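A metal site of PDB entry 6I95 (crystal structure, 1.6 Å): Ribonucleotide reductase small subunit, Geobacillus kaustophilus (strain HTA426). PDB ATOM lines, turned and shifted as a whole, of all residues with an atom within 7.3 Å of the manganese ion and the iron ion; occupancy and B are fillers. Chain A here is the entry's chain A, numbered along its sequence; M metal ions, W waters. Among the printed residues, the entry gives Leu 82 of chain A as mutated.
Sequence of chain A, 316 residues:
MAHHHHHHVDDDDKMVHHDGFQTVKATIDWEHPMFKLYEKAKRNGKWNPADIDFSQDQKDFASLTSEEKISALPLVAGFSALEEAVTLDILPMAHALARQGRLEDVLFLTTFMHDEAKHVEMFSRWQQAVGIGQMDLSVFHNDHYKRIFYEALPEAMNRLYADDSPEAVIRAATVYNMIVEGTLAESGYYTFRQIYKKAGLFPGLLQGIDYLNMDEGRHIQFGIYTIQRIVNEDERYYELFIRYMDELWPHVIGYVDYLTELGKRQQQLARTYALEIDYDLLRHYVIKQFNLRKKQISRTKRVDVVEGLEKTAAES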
ATOM      1  N   PHE A  79      12.101 -11.550   2.750  1.00  0.00           N
ATOM      2  CA  PHE A  79      11.886 -12.350   1.561  1.00  0.00           C
ATOM      3  C   PHE A  79      13.007 -13.343   1.314  1.00  0.00           C
ATOM      4  O   PHE A  79      12.740 -14.456   0.857  1.00  0.00           O
ATOM      5  CB  PHE A  79      11.706 -11.454   0.343  1.00  0.00           C
ATOM      6  CG  PHE A  79      10.296 -11.325  -0.068  1.00  0.00           C
ATOM      7  CD1 PHE A  79       9.598 -10.155   0.171  1.00  0.00           C
ATOM      8  CD2 PHE A  79       9.636 -12.395  -0.651  1.00  0.00           C
ATOM      9  CE1 PHE A  79       8.271 -10.031  -0.206  1.00  0.00           C
ATOM     10  CE2 PHE A  79       8.302 -12.279  -1.032  1.00  0.00           C
ATOM     11  CZ  PHE A  79       7.625 -11.095  -0.797  1.00  0.00           C
ATOM     12  N   LEU A  82      12.253 -16.193   3.545  1.00  0.00           N
ATOM     13  CA  LEU A  82      11.036 -16.889   3.122  1.00  0.00           C
ATOM     14  C   LEU A  82      11.339 -17.808   1.959  1.00  0.00           C
ATOM     15  O   LEU A  82      10.934 -18.980   1.953  1.00  0.00           O
ATOM     16  CB  LEU A  82       9.974 -15.871   2.731  1.00  0.00           C
ATOM     17  CG  LEU A  82       8.607 -16.426   2.365  1.00  0.00           C
ATOM     18  CD1 LEU A  82       7.546 -15.350   2.699  1.00  0.00           C
ATOM     19  CD2 LEU A  82       8.530 -16.842   0.933  1.00  0.00           C
ATOM     20  N   GLU A  83      12.041 -17.294   0.936  1.00  0.00           N
ATOM     21  CA  GLU A  83      12.277 -18.111  -0.249  1.00  0.00           C
ATOM     22  C   GLU A  83      13.213 -19.276   0.060  1.00  0.00           C
ATOM     23  O   GLU A  83      13.044 -20.373  -0.465  1.00  0.00           O
ATOM     24  CB  GLU A  83      12.850 -17.284  -1.402  1.00  0.00           C
ATOM     25  CG  GLU A  83      11.955 -16.081  -1.804  1.00  0.00           C
ATOM     26  CD  GLU A  83      10.579 -16.444  -2.370  1.00  0.00           C
ATOM     27  OE1 GLU A  83      10.351 -17.609  -2.799  1.00  0.00           O
ATOM     28  OE2 GLU A  83       9.704 -15.537  -2.354  1.00  0.00           O
ATOM     29  N   VAL A  86      11.048 -21.905   1.993  1.00  0.00           N
ATOM     30  CA  VAL A  86      10.121 -22.695   1.196  1.00  0.00           C
ATOM     31  C   VAL A  86      10.847 -23.569   0.191  1.00  0.00           C
ATOM     32  O   VAL A  86      10.297 -24.593  -0.245  1.00  0.00           O
ATOM     33  CB  VAL A  86       9.071 -21.812   0.491  1.00  0.00           C
ATOM     34  CG1 VAL A  86       8.219 -21.091   1.494  1.00  0.00           C
ATOM     35  CG2 VAL A  86       9.699 -20.792  -0.509  1.00  0.00           C
ATOM     36  N   THR A  87      12.072 -23.220  -0.225  1.00  0.00           N
ATOM     37  CA  THR A  87      12.810 -24.129  -1.099  1.00  0.00           C
ATOM     38  C   THR A  87      13.104 -25.419  -0.373  1.00  0.00           C
ATOM     39  O   THR A  87      12.887 -26.527  -0.907  1.00  0.00           O
ATOM     40  CB  THR A  87      14.130 -23.489  -1.571  1.00  0.00           C
ATOM     41  OG1 THR A  87      13.862 -22.327  -2.340  1.00  0.00           O
ATOM     42  CG2 THR A  87      14.924 -24.434  -2.466  1.00  0.00           C
ATOM     43  N   PHE A 112       7.610 -26.631  -8.879  1.00  0.00           N
ATOM     44  CA  PHE A 112       7.422 -25.797  -7.694  1.00  0.00           C
ATOM     45  C   PHE A 112       8.757 -25.568  -7.000  1.00  0.00           C
ATOM     46  O   PHE A 112       9.134 -24.415  -6.690  1.00  0.00           O
ATOM     47  CB  PHE A 112       6.393 -26.525  -6.810  1.00  0.00           C
ATOM     48  CG  PHE A 112       5.820 -25.755  -5.641  1.00  0.00           C
ATOM     49  CD1 PHE A 112       4.451 -25.759  -5.454  1.00  0.00           C
ATOM     50  CD2 PHE A 112       6.593 -25.143  -4.676  1.00  0.00           C
ATOM     51  CE1 PHE A 112       3.873 -25.105  -4.401  1.00  0.00           C
ATOM     52  CE2 PHE A 112       6.004 -24.486  -3.587  1.00  0.00           C
ATOM     53  CZ  PHE A 112       4.646 -24.482  -3.452  1.00  0.00           C
ATOM     54  N   ASP A 115      11.144 -23.452  -9.153  1.00  0.00           N
ATOM     55  CA  ASP A 115      10.728 -22.065  -9.043  1.00  0.00           C
ATOM     56  C   ASP A 115      11.298 -21.437  -7.771  1.00  0.00           C
ATOM     57  O   ASP A 115      11.865 -20.339  -7.804  1.00  0.00           O
ATOM     58  CB  ASP A 115       9.201 -21.913  -9.023  1.00  0.00           C
ATOM     59  CG  ASP A 115       8.528 -22.232 -10.312  1.00  0.00           C
ATOM     60  OD1 ASP A 115       9.167 -22.351 -11.367  1.00  0.00           O
ATOM     61  OD2 ASP A 115       7.283 -22.381 -10.278  1.00  0.00           O
ATOM     62  N   GLU A 116      11.123 -22.113  -6.619  1.00  0.00           N
ATOM     63  CA  GLU A 116      11.598 -21.520  -5.371  1.00  0.00           C
ATOM     64  C   GLU A 116      13.116 -21.324  -5.391  1.00  0.00           C
ATOM     65  O   GLU A 116      13.596 -20.318  -4.876  1.00  0.00           O
ATOM     66  CB  GLU A 116      11.256 -22.364  -4.138  1.00  0.00           C
ATOM     67  CG  GLU A 116       9.768 -22.632  -3.974  1.00  0.00           C
ATOM     68  CD  GLU A 116       8.904 -21.412  -3.839  1.00  0.00           C
ATOM     69  OE1 GLU A 116       9.356 -20.234  -3.885  1.00  0.00           O
ATOM     70  OE2 GLU A 116       7.715 -21.656  -3.615  1.00  0.00           O
ATOM     71  N   ALA A 117      13.857 -22.245  -5.993  1.00  0.00           N
ATOM     72  CA  ALA A 117      15.311 -22.072  -6.146  1.00  0.00           C
ATOM     73  C   ALA A 117      15.629 -20.785  -6.902  1.00  0.00           C
ATOM     74  O   ALA A 117      16.534 -20.014  -6.514  1.00  0.00           O
ATOM     75  CB  ALA A 117      15.891 -23.268  -6.906  1.00  0.00           C
ATOM     76  N   LYS A 118      14.907 -20.518  -8.002  1.00  0.00           N
ATOM     77  CA  LYS A 118      15.085 -19.246  -8.702  1.00  0.00           C
ATOM     78  C   LYS A 118      14.730 -18.059  -7.823  1.00  0.00           C
ATOM     79  O   LYS A 118      15.343 -16.974  -7.944  1.00  0.00           O
ATOM     80  CB  LYS A 118      14.237 -19.223  -9.987  1.00  0.00           C
ATOM     81  CG  LYS A 118      14.729 -20.254 -10.978  1.00  0.00           C
ATOM     82  CD  LYS A 118      14.140 -20.121 -12.400  1.00  0.00           C
ATOM     83  CE  LYS A 118      12.669 -20.273 -12.468  1.00  0.00           C
ATOM     84  NZ  LYS A 118      12.252 -20.280 -13.957  1.00  0.00           N
ATOM     85  N   HIS A 119      13.695 -18.174  -6.991  1.00  0.00           N
ATOM     86  CA  HIS A 119      13.328 -17.048  -6.138  1.00  0.00           C
ATOM     87  C   HIS A 119      14.424 -16.748  -5.128  1.00  0.00           C
ATOM     88  O   HIS A 119      14.760 -15.589  -4.910  1.00  0.00           O
ATOM     89  CB  HIS A 119      12.036 -17.331  -5.404  1.00  0.00           C
ATOM     90  CG  HIS A 119      10.894 -17.559  -6.325  1.00  0.00           C
ATOM     91  ND1 HIS A 119       9.638 -17.962  -5.895  1.00  0.00           N
ATOM     92  CD2 HIS A 119      10.844 -17.522  -7.670  1.00  0.00           C
ATOM     93  CE1 HIS A 119       8.870 -18.156  -6.947  1.00  0.00           C
ATOM     94  NE2 HIS A 119       9.571 -17.893  -8.039  1.00  0.00           N
ATOM     95  N   VAL A 120      14.979 -17.792  -4.502  1.00  0.00           N
ATOM     96  CA  VAL A 120      16.126 -17.611  -3.585  1.00  0.00           C
ATOM     97  C   VAL A 120      17.259 -16.924  -4.315  1.00  0.00           C
ATOM     98  O   VAL A 120      17.911 -15.977  -3.806  1.00  0.00           O
ATOM     99  CB  VAL A 120      16.610 -18.972  -3.035  1.00  0.00           C
ATOM    100  CG1 VAL A 120      17.906 -18.808  -2.159  1.00  0.00           C
ATOM    101  CG2 VAL A 120      15.566 -19.610  -2.250  1.00  0.00           C
ATOM    102  N   PHE A 123      16.786 -12.965  -5.075  1.00  0.00           N
ATOM    103  CA  PHE A 123      17.023 -12.014  -3.993  1.00  0.00           C
ATOM    104  C   PHE A 123      18.498 -11.993  -3.606  1.00  0.00           C
ATOM    105  O   PHE A 123      19.023 -10.931  -3.242  1.00  0.00           O
ATOM    106  CB  PHE A 123      16.177 -12.353  -2.788  1.00  0.00           C
ATOM    107  CG  PHE A 123      14.747 -11.949  -2.952  1.00  0.00           C
ATOM    108  CD1 PHE A 123      14.380 -10.631  -2.965  1.00  0.00           C
ATOM    109  CD2 PHE A 123      13.775 -12.928  -3.082  1.00  0.00           C
ATOM    110  CE1 PHE A 123      13.028 -10.273  -3.142  1.00  0.00           C
ATOM    111  CE2 PHE A 123      12.452 -12.594  -3.238  1.00  0.00           C
ATOM    112  CZ  PHE A 123      12.086 -11.255  -3.285  1.00  0.00           C
ATOM    113  N   TYR A 176       2.181 -23.719   4.787  1.00  0.00           N
ATOM    114  CA  TYR A 176       3.080 -23.430   3.682  1.00  0.00           C
ATOM    115  C   TYR A 176       2.384 -22.587   2.614  1.00  0.00           C
ATOM    116  O   TYR A 176       2.837 -21.484   2.289  1.00  0.00           O
ATOM    117  CB  TYR A 176       3.588 -24.733   3.054  1.00  0.00           C
ATOM    118  CG  TYR A 176       4.695 -24.601   2.047  1.00  0.00           C
ATOM    119  CD1 TYR A 176       5.919 -25.197   2.265  1.00  0.00           C
ATOM    120  CD2 TYR A 176       4.514 -23.913   0.856  1.00  0.00           C
ATOM    121  CE1 TYR A 176       6.950 -25.143   1.326  1.00  0.00           C
ATOM    122  CE2 TYR A 176       5.539 -23.856  -0.104  1.00  0.00           C
ATOM    123  CZ  TYR A 176       6.747 -24.461   0.153  1.00  0.00           C
ATOM    124  OH  TYR A 176       7.779 -24.420  -0.793  1.00  0.00           O
ATOM    125  N   ASN A 177       1.277 -23.089   2.079  1.00  0.00           N
ATOM    126  CA  ASN A 177       0.712 -22.475   0.889  1.00  0.00           C
ATOM    127  C   ASN A 177      -0.229 -21.338   1.239  1.00  0.00           C
ATOM    128  O   ASN A 177      -0.252 -20.320   0.544  1.00  0.00           O
ATOM    129  CB  ASN A 177      -0.042 -23.489   0.044  1.00  0.00           C
ATOM    130  CG  ASN A 177       0.816 -24.642  -0.401  1.00  0.00           C
ATOM    131  OD1 ASN A 177       0.863 -25.686   0.233  1.00  0.00           O
ATOM    132  ND2 ASN A 177       1.493 -24.459  -1.519  1.00  0.00           N
ATOM    133  N   GLU A 181       2.979 -18.502   1.823  1.00  0.00           N
ATOM    134  CA  GLU A 181       2.952 -17.993   0.447  1.00  0.00           C
ATOM    135  C   GLU A 181       1.709 -17.141   0.197  1.00  0.00           C
ATOM    136  O   GLU A 181       1.819 -16.043  -0.341  1.00  0.00           O
ATOM    137  CB  GLU A 181       3.028 -19.138  -0.555  1.00  0.00           C
ATOM    138  CG  GLU A 181       4.313 -20.024  -0.335  1.00  0.00           C
ATOM    139  CD  GLU A 181       4.982 -20.439  -1.638  1.00  0.00           C
ATOM    140  OE1 GLU A 181       6.006 -19.815  -2.000  1.00  0.00           O
ATOM    141  OE2 GLU A 181       4.476 -21.305  -2.339  1.00  0.00           O
ATOM    142  N   ALA A 185       3.747 -13.802   1.712  1.00  0.00           N
ATOM    143  CA  ALA A 185       4.481 -13.476   0.496  1.00  0.00           C
ATOM    144  C   ALA A 185       3.630 -12.633  -0.449  1.00  0.00           C
ATOM    145  O   ALA A 185       4.120 -11.644  -1.017  1.00  0.00           O
ATOM    146  CB  ALA A 185       4.971 -14.741  -0.215  1.00  0.00           C
ATOM    147  N   TYR A 189       4.971  -8.975  -1.788  1.00  0.00           N
ATOM    148  CA  TYR A 189       5.105  -8.551  -3.187  1.00  0.00           C
ATOM    149  C   TYR A 189       4.392  -7.242  -3.379  1.00  0.00           C
ATOM    150  O   TYR A 189       4.963  -6.248  -3.837  1.00  0.00           O
ATOM    151  CB  TYR A 189       4.463  -9.532  -4.195  1.00  0.00           C
ATOM    152  CG  TYR A 189       4.776 -10.979  -4.064  1.00  0.00           C
ATOM    153  CD1 TYR A 189       5.992 -11.403  -3.592  1.00  0.00           C
ATOM    154  CD2 TYR A 189       3.826 -11.941  -4.440  1.00  0.00           C
ATOM    155  CE1 TYR A 189       6.256 -12.734  -3.462  1.00  0.00           C
ATOM    156  CE2 TYR A 189       4.091 -13.266  -4.319  1.00  0.00           C
ATOM    157  CZ  TYR A 189       5.309 -13.654  -3.836  1.00  0.00           C
ATOM    158  OH  TYR A 189       5.586 -14.989  -3.697  1.00  0.00           O
ATOM    159  N   LEU A 212       8.393 -13.698 -10.175  1.00  0.00           N
ATOM    160  CA  LEU A 212       8.118 -14.517  -9.007  1.00  0.00           C
ATOM    161  C   LEU A 212       6.616 -14.616  -8.741  1.00  0.00           C
ATOM    162  O   LEU A 212       6.081 -15.698  -8.475  1.00  0.00           O
ATOM    163  CB  LEU A 212       8.874 -13.931  -7.836  1.00  0.00           C
ATOM    164  CG  LEU A 212       8.889 -14.506  -6.477  1.00  0.00           C
ATOM    165  CD1 LEU A 212      10.115 -13.917  -5.733  1.00  0.00           C
ATOM    166  CD2 LEU A 212       7.619 -14.083  -5.819  1.00  0.00           C
ATOM    167  N   ASP A 215       4.981 -17.102 -10.955  1.00  0.00           N
ATOM    168  CA  ASP A 215       5.217 -18.472 -10.488  1.00  0.00           C
ATOM    169  C   ASP A 215       4.290 -18.806  -9.342  1.00  0.00           C
ATOM    170  O   ASP A 215       3.720 -19.898  -9.293  1.00  0.00           O
ATOM    171  CB  ASP A 215       6.667 -18.681 -10.031  1.00  0.00           C
ATOM    172  CG  ASP A 215       7.705 -18.551 -11.123  1.00  0.00           C
ATOM    173  OD1 ASP A 215       7.426 -18.771 -12.326  1.00  0.00           O
ATOM    174  OD2 ASP A 215       8.877 -18.248 -10.739  1.00  0.00           O
ATOM    175  N   GLU A 216       4.150 -17.887  -8.384  1.00  0.00           N
ATOM    176  CA  GLU A 216       3.445 -18.185  -7.138  1.00  0.00           C
ATOM    177  C   GLU A 216       1.958 -18.359  -7.383  1.00  0.00           C
ATOM    178  O   GLU A 216       1.289 -19.021  -6.589  1.00  0.00           O
ATOM    179  CB  GLU A 216       3.747 -17.117  -6.123  1.00  0.00           C
ATOM    180  CG  GLU A 216       5.215 -17.181  -5.706  1.00  0.00           C
ATOM    181  CD  GLU A 216       5.568 -18.452  -4.954  1.00  0.00           C
ATOM    182  OE1 GLU A 216       4.650 -19.028  -4.349  1.00  0.00           O
ATOM    183  OE2 GLU A 216       6.767 -18.802  -4.974  1.00  0.00           O
ATOM    184  N   GLY A 217       1.436 -17.821  -8.489  1.00  0.00           N
ATOM    185  CA  GLY A 217       0.076 -18.152  -8.895  1.00  0.00           C
ATOM    186  C   GLY A 217      -0.157 -19.644  -9.054  1.00  0.00           C
ATOM    187  O   GLY A 217      -1.186 -20.169  -8.608  1.00  0.00           O
ATOM    188  N   ARG A 218       0.791 -20.359  -9.664  1.00  0.00           N
ATOM    189  CA  ARG A 218       0.648 -21.803  -9.767  1.00  0.00           C
ATOM    190  C   ARG A 218       0.774 -22.472  -8.415  1.00  0.00           C
ATOM    191  O   ARG A 218       0.066 -23.435  -8.118  1.00  0.00           O
ATOM    192  CB  ARG A 218       1.681 -22.408 -10.717  1.00  0.00           C
ATOM    193  CG  ARG A 218       1.644 -21.915 -12.127  1.00  0.00           C
ATOM    194  CD  ARG A 218       2.573 -22.750 -12.985  1.00  0.00           C
ATOM    195  NE  ARG A 218       3.973 -22.499 -12.603  1.00  0.00           N
ATOM    196  CZ  ARG A 218       4.669 -21.447 -13.022  1.00  0.00           C
ATOM    197  NH1 ARG A 218       4.132 -20.569 -13.853  1.00  0.00           N
ATOM    198  NH2 ARG A 218       5.927 -21.291 -12.619  1.00  0.00           N
ATOM    199  N   HIS A 219       1.721 -22.011  -7.593  1.00  0.00           N
ATOM    200  CA  HIS A 219       1.954 -22.664  -6.320  1.00  0.00           C
ATOM    201  C   HIS A 219       0.702 -22.653  -5.455  1.00  0.00           C
ATOM    202  O   HIS A 219       0.382 -23.650  -4.781  1.00  0.00           O
ATOM    203  CB  HIS A 219       3.091 -21.990  -5.563  1.00  0.00           C
ATOM    204  CG  HIS A 219       4.391 -22.047  -6.280  1.00  0.00           C
ATOM    205  ND1 HIS A 219       5.564 -21.590  -5.722  1.00  0.00           N
ATOM    206  CD2 HIS A 219       4.696 -22.455  -7.532  1.00  0.00           C
ATOM    207  CE1 HIS A 219       6.537 -21.712  -6.606  1.00  0.00           C
ATOM    208  NE2 HIS A 219       6.041 -22.243  -7.712  1.00  0.00           N
ATOM    209  N   ILE A 220      -0.030 -21.540  -5.450  1.00  0.00           N
ATOM    210  CA  ILE A 220      -1.204 -21.469  -4.580  1.00  0.00           C
ATOM    211  C   ILE A 220      -2.294 -22.402  -5.084  1.00  0.00           C
ATOM    212  O   ILE A 220      -3.041 -22.956  -4.285  1.00  0.00           O
ATOM    213  CB  ILE A 220      -1.695 -20.000  -4.448  1.00  0.00           C
ATOM    214  CG1 ILE A 220      -2.815 -19.921  -3.408  1.00  0.00           C
ATOM    215  CG2 ILE A 220      -2.208 -19.480  -5.774  1.00  0.00           C
ATOM    216  CD1 ILE A 220      -2.250 -20.086  -1.994  1.00  0.00           C
HETATM  217 MN    MN M   1       8.749 -18.273  -3.997  1.00  0.00          MN
HETATM  218 FE    FE M   2       5.933 -20.623  -3.820  1.00  0.00          FE
HETATM  219  O   HOH W   1       7.806 -16.372  -3.548  1.00  0.00           O
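The iron ion is bound by OE1 of Glu 181, at 2.0 Å.
OE2 of Glu 116 binds the iron ion, at 2.1 Å.
OE1 of Glu 216 binds the iron ion (2.1 Å).
The iron ion is bound by ND1 of His 219.
OE2 of Glu 181 is bound to the iron ion, 2.2 Å away.
The side-chain carboxylate (OE2) of Glu 216 is bound to the iron ion (2.3 Å).
Within 4 Å of the manganese ion: Glu 83, Glu 116, His 119, Glu 181 and Glu 216.
Residues that only touch the iron ion: Phe 112.
Five residues have an atom within 4 Å of the iron ion: Phe 112, Glu 116, Glu 181, Glu 216 and His 219.
The manganese ion is bound by OE1 of Glu 116 (2.1 Å).
The manganese ion is bound by OE1 of Glu 83 (2.1 Å).
A ring nitrogen (ND1) of His 119 is bound to the manganese ion, 2.1 Å away.
Water W1 is bound to the manganese ion.
The manganese ion is bound by OE2 of Glu 216 (2.3 Å).
The side-chain hydroxyl (OG1) of Thr 87 sits close to the backbone carbonyl oxygen (O) of Glu 116 (3.2 Å).
The side-chain carboxylate (OD2) of Asp 215 sits at hydrogen-bond distance from a ring nitrogen (NE2) of His 119 (2.8 Å).
The backbone NH of Glu 181 lies within hydrogen-bond range of the backbone carbonyl oxygen of Tyr 176.
O of Glu 83 lies within hydrogen-bond range of OG1 of Thr 87 (2.8 Å).
A ring nitrogen (NE2) of His 219 sits at hydrogen-bond distance from the side-chain carboxylate (OD2) of Asp 115, at 2.9 Å.
A ring nitrogen (NE2) of His 119 lies close to the backbone carbonyl oxygen (O) of Asp 115.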
